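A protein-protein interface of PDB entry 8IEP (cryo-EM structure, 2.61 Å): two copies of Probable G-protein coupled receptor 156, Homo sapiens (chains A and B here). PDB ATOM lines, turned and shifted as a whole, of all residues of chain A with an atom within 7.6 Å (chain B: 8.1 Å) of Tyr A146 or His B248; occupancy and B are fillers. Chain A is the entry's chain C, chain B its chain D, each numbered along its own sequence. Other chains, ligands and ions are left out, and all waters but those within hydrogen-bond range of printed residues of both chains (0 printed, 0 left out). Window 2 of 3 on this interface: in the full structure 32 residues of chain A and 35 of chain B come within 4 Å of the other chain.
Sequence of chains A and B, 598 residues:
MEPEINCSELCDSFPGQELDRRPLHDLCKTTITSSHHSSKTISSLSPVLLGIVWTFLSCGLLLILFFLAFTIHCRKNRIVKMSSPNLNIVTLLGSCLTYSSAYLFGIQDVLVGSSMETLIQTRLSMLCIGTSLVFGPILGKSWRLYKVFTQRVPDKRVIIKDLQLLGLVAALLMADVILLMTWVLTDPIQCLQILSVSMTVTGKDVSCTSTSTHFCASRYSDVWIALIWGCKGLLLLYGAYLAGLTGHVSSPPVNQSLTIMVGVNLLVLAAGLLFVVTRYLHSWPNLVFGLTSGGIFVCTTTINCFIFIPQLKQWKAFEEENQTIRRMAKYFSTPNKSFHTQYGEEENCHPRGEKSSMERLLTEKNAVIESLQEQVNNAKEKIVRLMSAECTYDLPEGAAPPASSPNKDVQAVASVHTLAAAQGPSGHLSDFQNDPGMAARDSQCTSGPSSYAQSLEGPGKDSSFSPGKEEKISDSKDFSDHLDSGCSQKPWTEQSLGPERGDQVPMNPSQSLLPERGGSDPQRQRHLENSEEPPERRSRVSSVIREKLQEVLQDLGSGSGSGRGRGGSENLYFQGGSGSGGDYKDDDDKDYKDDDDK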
ATOM      1  N   GLY A 140      -4.679  14.831 -20.681  1.00  0.00           N
ATOM      2  CA  GLY A 140      -5.572  15.368 -19.666  1.00  0.00           C
ATOM      3  C   GLY A 140      -5.143  15.003 -18.257  1.00  0.00           C
ATOM      4  O   GLY A 140      -5.204  15.831 -17.344  1.00  0.00           O
ATOM      5  N   LYS A 141      -4.706  13.758 -18.060  1.00  0.00           N
ATOM      6  CA  LYS A 141      -4.215  13.342 -16.751  1.00  0.00           C
ATOM      7  C   LYS A 141      -2.990  14.148 -16.342  1.00  0.00           C
ATOM      8  O   LYS A 141      -2.891  14.610 -15.197  1.00  0.00           O
ATOM      9  CB  LYS A 141      -3.884  11.852 -16.771  1.00  0.00           C
ATOM     10  CG  LYS A 141      -5.098  10.946 -16.686  1.00  0.00           C
ATOM     11  CD  LYS A 141      -4.711   9.508 -16.391  1.00  0.00           C
ATOM     12  CE  LYS A 141      -4.246   8.784 -17.633  1.00  0.00           C
ATOM     13  NZ  LYS A 141      -3.733   7.427 -17.309  1.00  0.00           N
ATOM     14  N   SER A 142      -2.044  14.331 -17.266  1.00  0.00           N
ATOM     15  CA  SER A 142      -0.857  15.120 -16.950  1.00  0.00           C
ATOM     16  C   SER A 142      -1.222  16.565 -16.639  1.00  0.00           C
ATOM     17  O   SER A 142      -0.650  17.172 -15.727  1.00  0.00           O
ATOM     18  CB  SER A 142       0.142  15.057 -18.102  1.00  0.00           C
ATOM     19  OG  SER A 142       0.729  13.774 -18.188  1.00  0.00           O
ATOM     20  N   TRP A 143      -2.170  17.134 -17.385  1.00  0.00           N
ATOM     21  CA  TRP A 143      -2.583  18.509 -17.130  1.00  0.00           C
ATOM     22  C   TRP A 143      -3.233  18.645 -15.760  1.00  0.00           C
ATOM     23  O   TRP A 143      -2.977  19.617 -15.041  1.00  0.00           O
ATOM     24  CB  TRP A 143      -3.536  18.978 -18.226  1.00  0.00           C
ATOM     25  CG  TRP A 143      -3.824  20.443 -18.177  1.00  0.00           C
ATOM     26  CD1 TRP A 143      -2.984  21.457 -18.529  1.00  0.00           C
ATOM     27  CD2 TRP A 143      -5.042  21.062 -17.750  1.00  0.00           C
ATOM     28  NE1 TRP A 143      -3.601  22.668 -18.347  1.00  0.00           N
ATOM     29  CE2 TRP A 143      -4.867  22.452 -17.872  1.00  0.00           C
ATOM     30  CE3 TRP A 143      -6.263  20.574 -17.279  1.00  0.00           C
ATOM     31  CZ2 TRP A 143      -5.866  23.359 -17.537  1.00  0.00           C
ATOM     32  CZ3 TRP A 143      -7.252  21.475 -16.948  1.00  0.00           C
ATOM     33  CH2 TRP A 143      -7.049  22.852 -17.079  1.00  0.00           C
ATOM     34  N   ARG A 144      -4.079  17.686 -15.379  1.00  0.00           N
ATOM     35  CA  ARG A 144      -4.693  17.741 -14.057  1.00  0.00           C
ATOM     36  C   ARG A 144      -3.652  17.603 -12.954  1.00  0.00           C
ATOM     37  O   ARG A 144      -3.735  18.289 -11.928  1.00  0.00           O
ATOM     38  CB  ARG A 144      -5.753  16.655 -13.917  1.00  0.00           C
ATOM     39  CG  ARG A 144      -6.632  16.834 -12.695  1.00  0.00           C
ATOM     40  CD  ARG A 144      -7.902  16.023 -12.798  1.00  0.00           C
ATOM     41  NE  ARG A 144      -7.620  14.595 -12.869  1.00  0.00           N
ATOM     42  CZ  ARG A 144      -8.473  13.675 -13.297  1.00  0.00           C
ATOM     43  NH1 ARG A 144      -9.691  13.991 -13.708  1.00  0.00           N
ATOM     44  NH2 ARG A 144      -8.096  12.400 -13.315  1.00  0.00           N
ATOM     45  N   LEU A 145      -2.681  16.705 -13.134  1.00  0.00           N
ATOM     46  CA  LEU A 145      -1.616  16.573 -12.144  1.00  0.00           C
ATOM     47  C   LEU A 145      -0.837  17.875 -12.011  1.00  0.00           C
ATOM     48  O   LEU A 145      -0.514  18.308 -10.898  1.00  0.00           O
ATOM     49  CB  LEU A 145      -0.688  15.423 -12.531  1.00  0.00           C
ATOM     50  CG  LEU A 145       0.312  14.940 -11.477  1.00  0.00           C
ATOM     51  CD1 LEU A 145      -0.393  14.353 -10.265  1.00  0.00           C
ATOM     52  CD2 LEU A 145       1.260  13.923 -12.086  1.00  0.00           C
ATOM     53  N   TYR A 146      -0.537  18.521 -13.138  1.00  0.00           N
ATOM     54  CA  TYR A 146       0.164  19.798 -13.097  1.00  0.00           C
ATOM     55  C   TYR A 146      -0.664  20.859 -12.384  1.00  0.00           C
ATOM     56  O   TYR A 146      -0.125  21.655 -11.606  1.00  0.00           O
ATOM     57  CB  TYR A 146       0.501  20.247 -14.517  1.00  0.00           C
ATOM     58  CG  TYR A 146       1.010  21.662 -14.614  1.00  0.00           C
ATOM     59  CD1 TYR A 146       2.225  22.020 -14.053  1.00  0.00           C
ATOM     60  CD2 TYR A 146       0.284  22.636 -15.279  1.00  0.00           C
ATOM     61  CE1 TYR A 146       2.697  23.308 -14.142  1.00  0.00           C
ATOM     62  CE2 TYR A 146       0.749  23.928 -15.374  1.00  0.00           C
ATOM     63  CZ  TYR A 146       1.957  24.258 -14.803  1.00  0.00           C
ATOM     64  OH  TYR A 146       2.428  25.546 -14.894  1.00  0.00           O
ATOM     65  N   LYS A 147      -1.973  20.892 -12.638  1.00  0.00           N
ATOM     66  CA  LYS A 147      -2.807  21.939 -12.057  1.00  0.00           C
ATOM     67  C   LYS A 147      -2.978  21.749 -10.555  1.00  0.00           C
ATOM     68  O   LYS A 147      -2.945  22.725  -9.798  1.00  0.00           O
ATOM     69  CB  LYS A 147      -4.170  21.977 -12.750  1.00  0.00           C
ATOM     70  CG  LYS A 147      -4.165  22.553 -14.171  1.00  0.00           C
ATOM     71  CD  LYS A 147      -3.757  24.029 -14.260  1.00  0.00           C
ATOM     72  CE  LYS A 147      -4.768  24.970 -13.618  1.00  0.00           C
ATOM     73  NZ  LYS A 147      -6.078  24.973 -14.322  1.00  0.00           N
ATOM     74  N   VAL A 148      -3.171  20.510 -10.099  1.00  0.00           N
ATOM     75  CA  VAL A 148      -3.259  20.287  -8.657  1.00  0.00           C
ATOM     76  C   VAL A 148      -1.916  20.515  -7.972  1.00  0.00           C
ATOM     77  O   VAL A 148      -1.886  21.046  -6.857  1.00  0.00           O
ATOM     78  CB  VAL A 148      -3.795  18.884  -8.315  1.00  0.00           C
ATOM     79  CG1 VAL A 148      -5.176  18.686  -8.916  1.00  0.00           C
ATOM     80  CG2 VAL A 148      -2.848  17.789  -8.775  1.00  0.00           C
ATOM     81  N   PHE A 149      -0.804  20.132  -8.604  1.00  0.00           N
ATOM     82  CA  PHE A 149       0.506  20.410  -8.029  1.00  0.00           C
ATOM     83  C   PHE A 149       0.772  21.907  -7.917  1.00  0.00           C
ATOM     84  O   PHE A 149       1.334  22.363  -6.916  1.00  0.00           O
ATOM     85  CB  PHE A 149       1.594  19.749  -8.878  1.00  0.00           C
ATOM     86  CG  PHE A 149       2.967  19.790  -8.260  1.00  0.00           C
ATOM     87  CD1 PHE A 149       3.209  19.229  -7.017  1.00  0.00           C
ATOM     88  CD2 PHE A 149       4.019  20.391  -8.932  1.00  0.00           C
ATOM     89  CE1 PHE A 149       4.475  19.266  -6.458  1.00  0.00           C
ATOM     90  CE2 PHE A 149       5.283  20.432  -8.376  1.00  0.00           C
ATOM     91  CZ  PHE A 149       5.509  19.869  -7.137  1.00  0.00           C
ATOM     92  N   THR A 150       0.390  22.681  -8.934  1.00  0.00           N
ATOM     93  CA  THR A 150       0.722  24.105  -9.005  1.00  0.00           C
ATOM     94  C   THR A 150      -0.501  24.937  -8.625  1.00  0.00           C
ATOM     95  O   THR A 150      -1.227  25.452  -9.475  1.00  0.00           O
ATOM     96  CB  THR A 150       1.226  24.465 -10.398  1.00  0.00           C
ATOM     97  OG1 THR A 150       0.372  23.873 -11.384  1.00  0.00           O
ATOM     98  CG2 THR A 150       2.647  23.966 -10.595  1.00  0.00           C
ATOM     99  N   GLN A 151      -0.714  25.077  -7.315  1.00  0.00           N
ATOM    100  CA  GLN A 151      -1.678  26.025  -6.754  1.00  0.00           C
ATOM    101  C   GLN A 151      -3.086  25.774  -7.306  1.00  0.00           C
ATOM    102  O   GLN A 151      -3.660  26.588  -8.033  1.00  0.00           O
ATOM    103  CB  GLN A 151      -1.234  27.468  -7.025  1.00  0.00           C
ATOM    104  CG  GLN A 151       0.099  27.842  -6.389  1.00  0.00           C
ATOM    105  CD  GLN A 151       0.053  27.820  -4.875  1.00  0.00           C
ATOM    106  OE1 GLN A 151       0.722  27.010  -4.235  1.00  0.00           O
ATOM    107  NE2 GLN A 151      -0.742  28.709  -4.294  1.00  0.00           N
ATOM    108  N   ARG A 152      -3.613  24.605  -6.950  1.00  0.00           N
ATOM    109  CA  ARG A 152      -4.940  24.171  -7.389  1.00  0.00           C
ATOM    110  C   ARG A 152      -6.017  25.229  -7.160  1.00  0.00           C
ATOM    111  O   ARG A 152      -6.729  25.615  -8.087  1.00  0.00           O
ATOM    112  CB  ARG A 152      -5.334  22.882  -6.665  1.00  0.00           C
ATOM    113  N   TYR A 238       3.036  19.693 -27.185  1.00  0.00           N
ATOM    114  CA  TYR A 238       2.449  20.130 -25.923  1.00  0.00           C
ATOM    115  C   TYR A 238       2.404  18.995 -24.906  1.00  0.00           C
ATOM    116  O   TYR A 238       2.583  19.231 -23.707  1.00  0.00           O
ATOM    117  CB  TYR A 238       1.050  20.697 -26.146  1.00  0.00           C
ATOM    118  CG  TYR A 238       0.436  21.265 -24.886  1.00  0.00           C
ATOM    119  CD1 TYR A 238       1.043  22.312 -24.208  1.00  0.00           C
ATOM    120  CD2 TYR A 238      -0.742  20.749 -24.370  1.00  0.00           C
ATOM    121  CE1 TYR A 238       0.491  22.830 -23.058  1.00  0.00           C
ATOM    122  CE2 TYR A 238      -1.301  21.261 -23.219  1.00  0.00           C
ATOM    123  CZ  TYR A 238      -0.680  22.300 -22.567  1.00  0.00           C
ATOM    124  OH  TYR A 238      -1.233  22.817 -21.420  1.00  0.00           O
ATOM    125  N   TYR A 241       5.791  18.730 -23.421  1.00  0.00           N
ATOM    126  CA  TYR A 241       5.934  19.816 -22.458  1.00  0.00           C
ATOM    127  C   TYR A 241       5.239  19.480 -21.142  1.00  0.00           C
ATOM    128  O   TYR A 241       5.787  19.718 -20.061  1.00  0.00           O
ATOM    129  CB  TYR A 241       5.370  21.103 -23.054  1.00  0.00           C
ATOM    130  CG  TYR A 241       5.544  22.329 -22.190  1.00  0.00           C
ATOM    131  CD1 TYR A 241       6.804  22.801 -21.867  1.00  0.00           C
ATOM    132  CD2 TYR A 241       4.443  23.021 -21.710  1.00  0.00           C
ATOM    133  CE1 TYR A 241       6.966  23.923 -21.085  1.00  0.00           C
ATOM    134  CE2 TYR A 241       4.596  24.142 -20.928  1.00  0.00           C
ATOM    135  CZ  TYR A 241       5.859  24.589 -20.618  1.00  0.00           C
ATOM    136  OH  TYR A 241       6.019  25.708 -19.837  1.00  0.00           O
ATOM    137  N   LEU A 242       4.029  18.921 -21.216  1.00  0.00           N
ATOM    138  CA  LEU A 242       3.312  18.524 -20.007  1.00  0.00           C
ATOM    139  C   LEU A 242       4.045  17.417 -19.261  1.00  0.00           C
ATOM    140  O   LEU A 242       4.104  17.426 -18.027  1.00  0.00           O
ATOM    141  CB  LEU A 242       1.897  18.066 -20.360  1.00  0.00           C
ATOM    142  CG  LEU A 242       0.809  19.132 -20.468  1.00  0.00           C
ATOM    143  CD1 LEU A 242      -0.457  18.513 -21.023  1.00  0.00           C
ATOM    144  CD2 LEU A 242       0.540  19.783 -19.123  1.00  0.00           C
ATOM    145  N   GLY A 244       7.216  16.915 -19.240  1.00  0.00           N
ATOM    146  CA  GLY A 244       8.319  17.568 -18.559  1.00  0.00           C
ATOM    147  C   GLY A 244       7.874  18.319 -17.320  1.00  0.00           C
ATOM    148  O   GLY A 244       8.535  18.263 -16.281  1.00  0.00           O
ATOM    149  N   LEU A 245       6.751  19.034 -17.411  1.00  0.00           N
ATOM    150  CA  LEU A 245       6.267  19.805 -16.269  1.00  0.00           C
ATOM    151  C   LEU A 245       5.955  18.902 -15.086  1.00  0.00           C
ATOM    152  O   LEU A 245       6.322  19.211 -13.947  1.00  0.00           O
ATOM    153  CB  LEU A 245       5.024  20.605 -16.658  1.00  0.00           C
ATOM    154  CG  LEU A 245       5.213  21.945 -17.370  1.00  0.00           C
ATOM    155  CD1 LEU A 245       3.868  22.477 -17.810  1.00  0.00           C
ATOM    156  CD2 LEU A 245       5.920  22.957 -16.488  1.00  0.00           C
ATOM    157  N   THR A 246       5.278  17.783 -15.334  1.00  0.00           N
ATOM    158  CA  THR A 246       4.967  16.815 -14.283  1.00  0.00           C
ATOM    159  C   THR A 246       6.059  15.747 -14.211  1.00  0.00           C
ATOM    160  O   THR A 246       5.801  14.547 -14.207  1.00  0.00           O
ATOM    161  CB  THR A 246       3.604  16.186 -14.539  1.00  0.00           C
ATOM    162  OG1 THR A 246       3.562  15.659 -15.869  1.00  0.00           O
ATOM    163  CG2 THR A 246       2.510  17.220 -14.391  1.00  0.00           C
ATOM    164  N   VAL A 249       7.100  14.143 -10.299  1.00  0.00           N
ATOM    165  CA  VAL A 249       6.141  14.796  -9.421  1.00  0.00           C
ATOM    166  C   VAL A 249       5.346  13.784  -8.605  1.00  0.00           C
ATOM    167  O   VAL A 249       4.829  14.117  -7.539  1.00  0.00           O
ATOM    168  CB  VAL A 249       5.210  15.712 -10.251  1.00  0.00           C
ATOM    169  CG1 VAL A 249       3.974  16.122  -9.462  1.00  0.00           C
ATOM    170  CG2 VAL A 249       5.969  16.948 -10.703  1.00  0.00           C
ATOM    171  N   LEU B 145      20.779  23.851 -16.932  1.00  0.00           N
ATOM    172  CA  LEU B 145      19.964  24.403 -15.854  1.00  0.00           C
ATOM    173  C   LEU B 145      19.237  23.299 -15.095  1.00  0.00           C
ATOM    174  O   LEU B 145      19.135  23.347 -13.865  1.00  0.00           O
ATOM    175  CB  LEU B 145      18.970  25.417 -16.422  1.00  0.00           C
ATOM    176  CG  LEU B 145      17.983  26.072 -15.452  1.00  0.00           C
ATOM    177  CD1 LEU B 145      18.717  26.998 -14.504  1.00  0.00           C
ATOM    178  CD2 LEU B 145      16.915  26.828 -16.218  1.00  0.00           C
ATOM    179  N   LEU B 242      12.583  19.064 -22.101  1.00  0.00           N
ATOM    180  CA  LEU B 242      13.499  19.857 -21.286  1.00  0.00           C
ATOM    181  C   LEU B 242      12.874  21.183 -20.869  1.00  0.00           C
ATOM    182  O   LEU B 242      13.078  21.643 -19.741  1.00  0.00           O
ATOM    183  CB  LEU B 242      14.797  20.108 -22.053  1.00  0.00           C
ATOM    184  CG  LEU B 242      15.861  19.013 -22.038  1.00  0.00           C
ATOM    185  CD1 LEU B 242      16.987  19.388 -22.981  1.00  0.00           C
ATOM    186  CD2 LEU B 242      16.395  18.780 -20.634  1.00  0.00           C
ATOM    187  N   ALA B 243      12.136  21.822 -21.776  1.00  0.00           N
ATOM    188  CA  ALA B 243      11.447  23.062 -21.437  1.00  0.00           C
ATOM    189  C   ALA B 243      10.415  22.828 -20.344  1.00  0.00           C
ATOM    190  O   ALA B 243      10.208  23.689 -19.481  1.00  0.00           O
ATOM    191  CB  ALA B 243      10.785  23.651 -22.680  1.00  0.00           C
ATOM    192  N   GLY B 244       9.741  21.679 -20.378  1.00  0.00           N
ATOM    193  CA  GLY B 244       8.838  21.336 -19.295  1.00  0.00           C
ATOM    194  C   GLY B 244       9.561  21.097 -17.984  1.00  0.00           C
ATOM    195  O   GLY B 244       9.095  21.519 -16.922  1.00  0.00           O
ATOM    196  N   LEU B 245      10.711  20.418 -18.036  1.00  0.00           N
ATOM    197  CA  LEU B 245      11.447  20.112 -16.812  1.00  0.00           C
ATOM    198  C   LEU B 245      11.904  21.373 -16.096  1.00  0.00           C
ATOM    199  O   LEU B 245      11.881  21.425 -14.862  1.00  0.00           O
ATOM    200  CB  LEU B 245      12.659  19.234 -17.120  1.00  0.00           C
ATOM    201  CG  LEU B 245      12.407  17.763 -17.448  1.00  0.00           C
ATOM    202  CD1 LEU B 245      13.648  17.164 -18.080  1.00  0.00           C
ATOM    203  CD2 LEU B 245      11.997  16.977 -16.216  1.00  0.00           C
ATOM    204  N   THR B 246      12.323  22.391 -16.844  1.00  0.00           N
ATOM    205  CA  THR B 246      12.770  23.668 -16.292  1.00  0.00           C
ATOM    206  C   THR B 246      11.691  24.732 -16.416  1.00  0.00           C
ATOM    207  O   THR B 246      11.990  25.898 -16.673  1.00  0.00           O
ATOM    208  CB  THR B 246      14.049  24.127 -16.987  1.00  0.00           C
ATOM    209  OG1 THR B 246      13.780  24.397 -18.368  1.00  0.00           O
ATOM    210  CG2 THR B 246      15.122  23.066 -16.890  1.00  0.00           C
ATOM    211  N   GLY B 247      10.429  24.346 -16.228  1.00  0.00           N
ATOM    212  CA  GLY B 247       9.328  25.243 -16.543  1.00  0.00           C
ATOM    213  C   GLY B 247       9.352  26.533 -15.747  1.00  0.00           C
ATOM    214  O   GLY B 247       9.150  27.615 -16.301  1.00  0.00           O
ATOM    215  N   HIS B 248       9.594  26.438 -14.443  1.00  0.00           N
ATOM    216  CA  HIS B 248       9.601  27.585 -13.541  1.00  0.00           C
ATOM    217  C   HIS B 248      10.804  27.516 -12.613  1.00  0.00           C
ATOM    218  O   HIS B 248      10.697  27.696 -11.398  1.00  0.00           O
ATOM    219  CB  HIS B 248       8.299  27.644 -12.749  1.00  0.00           C
ATOM    220  CG  HIS B 248       7.073  27.625 -13.607  1.00  0.00           C
ATOM    221  ND1 HIS B 248       6.703  28.690 -14.401  1.00  0.00           N
ATOM    222  CD2 HIS B 248       6.135  26.668 -13.801  1.00  0.00           C
ATOM    223  CE1 HIS B 248       5.590  28.389 -15.045  1.00  0.00           C
ATOM    224  NE2 HIS B 248       5.223  27.168 -14.699  1.00  0.00           N
ATOM    225  N   VAL B 249      11.976  27.254 -13.185  1.00  0.00           N
ATOM    226  CA  VAL B 249      13.187  27.068 -12.393  1.00  0.00           C
ATOM    227  C   VAL B 249      13.938  28.379 -12.197  1.00  0.00           C
ATOM    228  O   VAL B 249      14.651  28.545 -11.206  1.00  0.00           O
ATOM    229  CB  VAL B 249      14.076  25.993 -13.053  1.00  0.00           C
ATOM    230  CG1 VAL B 249      15.493  26.026 -12.498  1.00  0.00           C
ATOM    231  CG2 VAL B 249      13.470  24.621 -12.840  1.00  0.00           C
ATOM    232  N   SER B 250      13.815  29.330 -13.117  1.00  0.00           N
ATOM    233  CA  SER B 250      14.516  30.600 -12.979  1.00  0.00           C
ATOM    234  C   SER B 250      13.828  31.634 -13.864  1.00  0.00           C
ATOM    235  O   SER B 250      12.697  31.437 -14.318  1.00  0.00           O
ATOM    236  CB  SER B 250      16.002  30.427 -13.316  1.00  0.00           C
ATOM    237  OG  SER B 250      16.718  31.627 -13.084  1.00  0.00           O
ATOM    238  N   SER B 251      14.509  32.753 -14.087  1.00  0.00           N
ATOM    239  CA  SER B 251      13.978  33.841 -14.890  1.00  0.00           C
ATOM    240  C   SER B 251      14.144  33.555 -16.382  1.00  0.00           C
ATOM    241  O   SER B 251      14.923  32.683 -16.770  1.00  0.00           O
ATOM    242  CB  SER B 251      14.685  35.143 -14.535  1.00  0.00           C
ATOM    243  OG  SER B 251      14.516  35.464 -13.169  1.00  0.00           O
ATOM    244  N   ASN B 255      16.128  30.762 -17.704  1.00  0.00           N
ATOM    245  CA  ASN B 255      15.140  29.801 -18.165  1.00  0.00           C
ATOM    246  C   ASN B 255      14.849  30.012 -19.646  1.00  0.00           C
ATOM    247  O   ASN B 255      14.655  31.141 -20.098  1.00  0.00           O
ATOM    248  CB  ASN B 255      13.856  29.952 -17.350  1.00  0.00           C
ATOM    249  CG  ASN B 255      12.970  28.738 -17.423  1.00  0.00           C
ATOM    250  OD1 ASN B 255      13.351  27.709 -17.969  1.00  0.00           O
ATOM    251  ND2 ASN B 255      11.770  28.852 -16.874  1.00  0.00           N
ATOM    252  N   SER B 257      12.397  28.021 -21.392  1.00  0.00           N
ATOM    253  CA  SER B 257      11.226  27.213 -21.717  1.00  0.00           C
ATOM    254  C   SER B 257      10.333  27.901 -22.743  1.00  0.00           C
ATOM    255  O   SER B 257       9.895  27.272 -23.715  1.00  0.00           O
ATOM    256  CB  SER B 257      10.440  26.908 -20.445  1.00  0.00           C
ATOM    257  OG  SER B 257      11.241  26.204 -19.520  1.00  0.00           O
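Of chain B, only His B248 comes within 4 Å of Tyr A146. No residue of chain A comes within 4 Å of Gly B247. Of the printed residues of chain A, Ala B243 touches Tyr A241 (3.6 Å). Printed residues of chain A within 4 Å of Leu B245: Gly A244 (3.5 Å). Of the printed residues of chain B, Leu A245 touches Gly B244. The nearest residue of chain A that does not touch His B248 is Leu A245 (4.6 Å).
OH of Tyr A146 is in hydrogen-bond range of NE2 of His B248 (3.2 Å). O of Gly B244 lies close to N of Leu A245 (3.5 Å). O of Gly A244 lies close to O of Gly B244, at 3.4 Å.
Along chain B the printed residues that touch a printed residue of chain A span positions 243 to 248. Of the 20 printed residues of chain A, 4 touch a printed residue of chain B. Hydrophobic or aromatic side chains of chain A that line the printed part of chain B: Tyr A146, Tyr A241 and Leu A245. Among the printed residues, 6 pairs touch across the chains. Among the printed residues, no Asp or Glu carboxylate lies within 4 Å of a Lys or Arg side-chain nitrogen of the other chain.
The backbone carbonyl oxygen of Ala B243 is in hydrogen-bond range of the side-chain hydroxyl of Ser B257, at 2.7 Å.
Gly A244 touches its own counterpart, Gly B244. Gly A244 touches Leu B245, and with the chains exchanged Leu A245 touches Gly B244. Positions printed for both chains: 145, 242, 244, 245, 246 and 249.
Among the printed residues, pairs that only touch across the chains: Tyr A241 with Ala B243 (3.6 Å), Tyr A241 with Gly B244 (3.5 Å) and Gly A244 with Leu B245 (3.5 Å).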
